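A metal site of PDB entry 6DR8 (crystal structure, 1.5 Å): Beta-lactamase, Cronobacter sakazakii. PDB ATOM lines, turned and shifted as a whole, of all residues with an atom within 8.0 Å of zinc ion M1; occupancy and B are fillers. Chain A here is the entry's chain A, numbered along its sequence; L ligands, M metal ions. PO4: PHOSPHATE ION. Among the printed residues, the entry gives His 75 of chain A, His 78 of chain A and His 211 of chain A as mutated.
A ring nitrogen (ND1) of His 73 sits at hydrogen-bond distance from the side-chain carboxylate of Asp 170.
A ring nitrogen (ND1) of His 149 sits at hydrogen-bond distance from the backbone carbonyl oxygen (O) of Ala 173, at 2.7 Å.
OH of Tyr 177 sits at hydrogen-bond distance from O of His 149.
OD2 of Asp 110 is in hydrogen-bond range of NE2 of His 75, at 2.8 Å.
A ring nitrogen (ND1) of His 149 sits at hydrogen-bond distance from the side-chain hydroxyl (OG) of Ser 171 (3.3 Å).
Within 4 Å of zinc ion M1: His 73, His 75 and His 149.
Zinc ion M1 is bound by O2 of the ligand (1.9 Å), ND1 of His 75 (2.0 Å), NE2 of His 73 (2.0 Å) and NE2 of His 149 (2.0 Å).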
ATOM      1  N   SER A  72      -5.337 -14.412 -22.039  1.00  0.00           N
ATOM      2  CA  SER A  72      -5.750 -14.476 -20.639  1.00  0.00           C
ATOM      3  C   SER A  72      -6.611 -15.717 -20.389  1.00  0.00           C
ATOM      4  O   SER A  72      -6.211 -16.638 -19.665  1.00  0.00           O
ATOM      5  CB  SER A  72      -6.462 -13.177 -20.239  1.00  0.00           C
ATOM      6  OG  SER A  72      -7.599 -12.911 -21.041  1.00  0.00           O
ATOM      7  N   HIS A  73      -7.777 -15.793 -21.029  1.00  0.00           N
ATOM      8  CA  HIS A  73      -8.559 -17.027 -20.972  1.00  0.00           C
ATOM      9  C   HIS A  73      -9.390 -17.253 -22.241  1.00  0.00           C
ATOM     10  O   HIS A  73      -9.702 -16.331 -22.993  1.00  0.00           O
ATOM     11  CB  HIS A  73      -9.442 -17.119 -19.728  1.00  0.00           C
ATOM     12  CG  HIS A  73     -10.653 -16.233 -19.765  1.00  0.00           C
ATOM     13  ND1 HIS A  73     -10.651 -14.954 -19.257  1.00  0.00           N
ATOM     14  CD2 HIS A  73     -11.899 -16.449 -20.218  1.00  0.00           C
ATOM     15  CE1 HIS A  73     -11.847 -14.413 -19.409  1.00  0.00           C
ATOM     16  NE2 HIS A  73     -12.629 -15.300 -19.987  1.00  0.00           N
ATOM     17  N   ALA A  74      -9.769 -18.511 -22.428  1.00  0.00           N
ATOM     18  CA  ALA A  74     -10.289 -19.011 -23.703  1.00  0.00           C
ATOM     19  C   ALA A  74     -11.809 -18.872 -23.790  1.00  0.00           C
ATOM     20  O   ALA A  74     -12.538 -19.848 -24.022  1.00  0.00           O
ATOM     21  CB  ALA A  74      -9.887 -20.470 -23.875  1.00  0.00           C
ATOM     22  N   HIS A  75     -12.284 -17.636 -23.678  1.00  0.00           N
ATOM     23  CA  HIS A  75     -13.649 -17.253 -24.014  1.00  0.00           C
ATOM     24  C   HIS A  75     -13.640 -16.423 -25.293  1.00  0.00           C
ATOM     25  O   HIS A  75     -12.650 -15.792 -25.633  1.00  0.00           O
ATOM     26  CB  HIS A  75     -14.318 -16.489 -22.874  1.00  0.00           C
ATOM     27  CG  HIS A  75     -14.875 -17.386 -21.823  1.00  0.00           C
ATOM     28  ND1 HIS A  75     -15.150 -16.957 -20.539  1.00  0.00           N
ATOM     29  CD2 HIS A  75     -15.231 -18.686 -21.862  1.00  0.00           C
ATOM     30  CE1 HIS A  75     -15.639 -17.966 -19.840  1.00  0.00           C
ATOM     31  NE2 HIS A  75     -15.712 -19.024 -20.621  1.00  0.00           N
ATOM     32  N   LEU A  76     -14.796 -16.401 -25.964  1.00  0.00           N
ATOM     33  CA  LEU A  76     -14.876 -15.809 -27.298  1.00  0.00           C
ATOM     34  C   LEU A  76     -14.485 -14.339 -27.326  1.00  0.00           C
ATOM     35  O   LEU A  76     -14.056 -13.848 -28.376  1.00  0.00           O
ATOM     36  CB  LEU A  76     -16.270 -15.998 -27.892  1.00  0.00           C
ATOM     37  CG  LEU A  76     -17.394 -15.102 -27.399  1.00  0.00           C
ATOM     38  CD1 LEU A  76     -18.647 -15.326 -28.260  1.00  0.00           C
ATOM     39  CD2 LEU A  76     -17.716 -15.338 -25.942  1.00  0.00           C
ATOM     40  N   ASP A  77     -14.627 -13.617 -26.219  1.00  0.00           N
ATOM     41  CA  ASP A  77     -14.343 -12.191 -26.245  1.00  0.00           C
ATOM     42  C   ASP A  77     -12.884 -11.858 -25.991  1.00  0.00           C
ATOM     43  O   ASP A  77     -12.530 -10.684 -26.020  1.00  0.00           O
ATOM     44  CB  ASP A  77     -15.269 -11.416 -25.307  1.00  0.00           C
ATOM     45  CG  ASP A  77     -15.276 -11.943 -23.889  1.00  0.00           C
ATOM     46  OD1 ASP A  77     -15.076 -13.159 -23.660  1.00  0.00           O
ATOM     47  OD2 ASP A  77     -15.524 -11.119 -22.975  1.00  0.00           O
ATOM     48  N   HIS A  78     -12.020 -12.865 -25.776  1.00  0.00           N
ATOM     49  CA  HIS A  78     -10.578 -12.657 -25.638  1.00  0.00           C
ATOM     50  C   HIS A  78      -9.794 -13.508 -26.609  1.00  0.00           C
ATOM     51  O   HIS A  78      -8.747 -13.076 -27.091  1.00  0.00           O
ATOM     52  CB  HIS A  78     -10.143 -12.992 -24.205  1.00  0.00           C
ATOM     53  CG  HIS A  78     -10.953 -12.297 -23.160  1.00  0.00           C
ATOM     54  ND1 HIS A  78     -10.962 -10.927 -23.033  1.00  0.00           N
ATOM     55  CD2 HIS A  78     -11.835 -12.774 -22.249  1.00  0.00           C
ATOM     56  CE1 HIS A  78     -11.782 -10.587 -22.052  1.00  0.00           C
ATOM     57  NE2 HIS A  78     -12.324 -11.686 -21.561  1.00  0.00           N
ATOM     58  N   GLN A 102      -9.137 -25.617 -24.596  1.00  0.00           N
ATOM     59  CA  GLN A 102     -10.423 -25.004 -24.916  1.00  0.00           C
ATOM     60  C   GLN A 102     -10.360 -24.230 -26.235  1.00  0.00           C
ATOM     61  O   GLN A 102     -11.324 -24.250 -27.011  1.00  0.00           O
ATOM     62  CB  GLN A 102     -10.873 -24.126 -23.746  1.00  0.00           C
ATOM     63  CG  GLN A 102     -12.235 -23.487 -23.976  1.00  0.00           C
ATOM     64  CD  GLN A 102     -13.042 -23.320 -22.703  1.00  0.00           C
ATOM     65  OE1 GLN A 102     -13.177 -24.236 -21.903  1.00  0.00           O
ATOM     66  NE2 GLN A 102     -13.639 -22.155 -22.556  1.00  0.00           N
ATOM     67  N   ASP A 110     -17.013 -26.008 -22.557  1.00  0.00           N
ATOM     68  CA  ASP A 110     -16.780 -25.097 -21.445  1.00  0.00           C
ATOM     69  C   ASP A 110     -17.520 -25.611 -20.203  1.00  0.00           C
ATOM     70  O   ASP A 110     -18.665 -26.052 -20.288  1.00  0.00           O
ATOM     71  CB  ASP A 110     -17.303 -23.711 -21.857  1.00  0.00           C
ATOM     72  CG  ASP A 110     -17.034 -22.619 -20.833  1.00  0.00           C
ATOM     73  OD1 ASP A 110     -17.661 -22.640 -19.752  1.00  0.00           O
ATOM     74  OD2 ASP A 110     -16.221 -21.713 -21.115  1.00  0.00           O
ATOM     75  N   LEU A 113     -20.524 -23.100 -19.785  1.00  0.00           N
ATOM     76  CA  LEU A 113     -21.255 -22.707 -20.984  1.00  0.00           C
ATOM     77  C   LEU A 113     -21.526 -23.848 -21.947  1.00  0.00           C
ATOM     78  O   LEU A 113     -22.350 -23.681 -22.853  1.00  0.00           O
ATOM     79  CB  LEU A 113     -20.479 -21.614 -21.729  1.00  0.00           C
ATOM     80  CG  LEU A 113     -20.288 -20.301 -20.995  1.00  0.00           C
ATOM     81  CD1 LEU A 113     -19.318 -19.412 -21.758  1.00  0.00           C
ATOM     82  CD2 LEU A 113     -21.624 -19.608 -20.823  1.00  0.00           C
ATOM     83  N   HIS A 149     -12.197 -18.197 -12.817  1.00  0.00           N
ATOM     84  CA  HIS A 149     -13.107 -17.863 -13.909  1.00  0.00           C
ATOM     85  C   HIS A 149     -13.109 -18.980 -14.956  1.00  0.00           C
ATOM     86  O   HIS A 149     -14.157 -19.318 -15.520  1.00  0.00           O
ATOM     87  CB  HIS A 149     -12.682 -16.537 -14.531  1.00  0.00           C
ATOM     88  CG  HIS A 149     -13.539 -16.135 -15.679  1.00  0.00           C
ATOM     89  ND1 HIS A 149     -14.825 -15.657 -15.511  1.00  0.00           N
ATOM     90  CD2 HIS A 149     -13.324 -16.191 -17.011  1.00  0.00           C
ATOM     91  CE1 HIS A 149     -15.349 -15.398 -16.698  1.00  0.00           C
ATOM     92  NE2 HIS A 149     -14.455 -15.708 -17.627  1.00  0.00           N
ATOM     93  N   LEU A 150     -11.942 -19.543 -15.227  1.00  0.00           N
ATOM     94  CA  LEU A 150     -11.768 -20.781 -15.968  1.00  0.00           C
ATOM     95  C   LEU A 150     -10.602 -21.516 -15.332  1.00  0.00           C
ATOM     96  O   LEU A 150      -9.761 -20.903 -14.670  1.00  0.00           O
ATOM     97  CB  LEU A 150     -11.474 -20.576 -17.471  1.00  0.00           C
ATOM     98  CG  LEU A 150     -12.643 -20.232 -18.386  1.00  0.00           C
ATOM     99  CD1 LEU A 150     -12.115 -20.082 -19.797  1.00  0.00           C
ATOM    100  CD2 LEU A 150     -13.748 -21.305 -18.344  1.00  0.00           C
ATOM    101  N   ALA A 153      -7.330 -19.827 -16.467  1.00  0.00           N
ATOM    102  CA  ALA A 153      -7.231 -18.374 -16.518  1.00  0.00           C
ATOM    103  C   ALA A 153      -5.861 -17.907 -16.062  1.00  0.00           C
ATOM    104  O   ALA A 153      -5.310 -18.396 -15.072  1.00  0.00           O
ATOM    105  CB  ALA A 153      -8.328 -17.749 -15.657  1.00  0.00           C
ATOM    106  N   ASP A 170      -6.581 -11.045 -15.484  1.00  0.00           N
ATOM    107  CA  ASP A 170      -7.712 -11.771 -16.028  1.00  0.00           C
ATOM    108  C   ASP A 170      -8.991 -11.486 -15.219  1.00  0.00           C
ATOM    109  O   ASP A 170      -8.998 -10.800 -14.188  1.00  0.00           O
ATOM    110  CB  ASP A 170      -7.403 -13.257 -16.035  1.00  0.00           C
ATOM    111  CG  ASP A 170      -8.135 -14.026 -17.128  1.00  0.00           C
ATOM    112  OD1 ASP A 170      -9.138 -13.532 -17.701  1.00  0.00           O
ATOM    113  OD2 ASP A 170      -7.718 -15.174 -17.396  1.00  0.00           O
ATOM    114  N   SER A 171     -10.081 -12.023 -15.725  1.00  0.00           N
ATOM    115  CA  SER A 171     -11.355 -11.969 -15.044  1.00  0.00           C
ATOM    116  C   SER A 171     -11.302 -12.758 -13.741  1.00  0.00           C
ATOM    117  O   SER A 171     -10.738 -13.852 -13.665  1.00  0.00           O
ATOM    118  CB  SER A 171     -12.420 -12.571 -15.940  1.00  0.00           C
ATOM    119  OG  SER A 171     -13.692 -12.551 -15.313  1.00  0.00           O
ATOM    120  N   ALA A 173     -14.476 -12.961 -12.392  1.00  0.00           N
ATOM    121  CA  ALA A 173     -15.932 -13.053 -12.311  1.00  0.00           C
ATOM    122  C   ALA A 173     -16.387 -14.515 -12.378  1.00  0.00           C
ATOM    123  O   ALA A 173     -15.714 -15.381 -12.957  1.00  0.00           O
ATOM    124  CB  ALA A 173     -16.577 -12.251 -13.435  1.00  0.00           C
ATOM    125  N   PRO A 175     -19.871 -15.542 -13.268  1.00  0.00           N
ATOM    126  CA  PRO A 175     -21.274 -15.224 -13.637  1.00  0.00           C
ATOM    127  C   PRO A 175     -22.132 -16.476 -13.840  1.00  0.00           C
ATOM    128  O   PRO A 175     -21.912 -17.252 -14.774  1.00  0.00           O
ATOM    129  CB  PRO A 175     -21.123 -14.452 -14.953  1.00  0.00           C
ATOM    130  CG  PRO A 175     -19.891 -15.019 -15.539  1.00  0.00           C
ATOM    131  CD  PRO A 175     -18.958 -15.222 -14.375  1.00  0.00           C
ATOM    132  N   TYR A 177     -22.189 -19.099 -12.121  1.00  0.00           N
ATOM    133  CA  TYR A 177     -21.490 -20.359 -11.875  1.00  0.00           C
ATOM    134  C   TYR A 177     -22.051 -21.042 -10.634  1.00  0.00           C
ATOM    135  O   TYR A 177     -22.122 -20.413  -9.575  1.00  0.00           O
ATOM    136  CB  TYR A 177     -20.023 -20.111 -11.586  1.00  0.00           C
ATOM    137  CG  TYR A 177     -19.158 -19.712 -12.757  1.00  0.00           C
ATOM    138  CD1 TYR A 177     -19.702 -19.460 -14.012  1.00  0.00           C
ATOM    139  CD2 TYR A 177     -17.797 -19.604 -12.608  1.00  0.00           C
ATOM    140  CE1 TYR A 177     -18.893 -19.104 -15.084  1.00  0.00           C
ATOM    141  CE2 TYR A 177     -16.965 -19.235 -13.666  1.00  0.00           C
ATOM    142  CZ  TYR A 177     -17.519 -18.997 -14.897  1.00  0.00           C
ATOM    143  OH  TYR A 177     -16.697 -18.653 -15.931  1.00  0.00           O
ATOM    144  N   ASN A 210      -8.478  -7.360 -18.822  1.00  0.00           N
ATOM    145  CA  ASN A 210      -8.960  -7.787 -20.127  1.00  0.00           C
ATOM    146  C   ASN A 210     -10.332  -7.218 -20.483  1.00  0.00           C
ATOM    147  O   ASN A 210     -10.851  -7.514 -21.560  1.00  0.00           O
ATOM    148  CB  ASN A 210      -8.912  -9.307 -20.315  1.00  0.00           C
ATOM    149  CG  ASN A 210      -9.708 -10.055 -19.296  1.00  0.00           C
ATOM    150  OD1 ASN A 210     -10.391  -9.463 -18.475  1.00  0.00           O
ATOM    151  ND2 ASN A 210      -9.636 -11.378 -19.357  1.00  0.00           N
ATOM    152  N   HIS A 211     -10.907  -6.385 -19.612  1.00  0.00           N
ATOM    153  CA  HIS A 211     -12.086  -5.595 -19.936  1.00  0.00           C
ATOM    154  C   HIS A 211     -11.834  -4.180 -19.449  1.00  0.00           C
ATOM    155  O   HIS A 211     -11.351  -3.989 -18.323  1.00  0.00           O
ATOM    156  CB  HIS A 211     -13.338  -6.163 -19.248  1.00  0.00           C
ATOM    157  CG  HIS A 211     -14.141  -7.096 -20.105  1.00  0.00           C
ATOM    158  ND1 HIS A 211     -15.040  -6.663 -21.049  1.00  0.00           N
ATOM    159  CD2 HIS A 211     -14.160  -8.448 -20.170  1.00  0.00           C
ATOM    160  CE1 HIS A 211     -15.598  -7.698 -21.643  1.00  0.00           C
ATOM    161  NE2 HIS A 211     -15.072  -8.796 -21.134  1.00  0.00           N
ATOM    162  N   ARG A 214     -12.896  -2.938 -16.009  1.00  0.00           N
ATOM    163  CA  ARG A 214     -12.204  -3.498 -14.857  1.00  0.00           C
ATOM    164  C   ARG A 214     -11.005  -2.644 -14.413  1.00  0.00           C
ATOM    165  O   ARG A 214     -10.569  -2.763 -13.265  1.00  0.00           O
ATOM    166  CB  ARG A 214     -11.750  -4.923 -15.150  1.00  0.00           C
ATOM    167  CG  ARG A 214     -12.885  -5.894 -15.441  1.00  0.00           C
ATOM    168  CD  ARG A 214     -12.428  -7.328 -15.734  1.00  0.00           C
ATOM    169  NE  ARG A 214     -13.608  -8.186 -15.733  1.00  0.00           N
ATOM    170  CZ  ARG A 214     -13.852  -9.191 -16.572  1.00  0.00           C
ATOM    171  NH1 ARG A 214     -13.003  -9.528 -17.530  1.00  0.00           N
ATOM    172  NH2 ARG A 214     -15.001  -9.831 -16.445  1.00  0.00           N
HETATM  173  P   PO4 L   1     -15.154 -12.235 -19.329  1.00  0.00           P
HETATM  174  O1  PO4 L   1     -16.062 -11.272 -20.068  1.00  0.00           O
HETATM  175  O2  PO4 L   1     -15.377 -13.601 -19.928  1.00  0.00           O
HETATM  176  O3  PO4 L   1     -13.710 -11.792 -19.454  1.00  0.00           O
HETATM  177  O4  PO4 L   1     -15.482 -12.188 -17.846  1.00  0.00           O
HETATM  178 ZN    ZN M   1     -14.603 -15.295 -19.599  1.00  0.00          ZN
HETATM  179 ZN    ZN M   2     -14.263 -11.123 -21.149  1.00  0.00          ZN
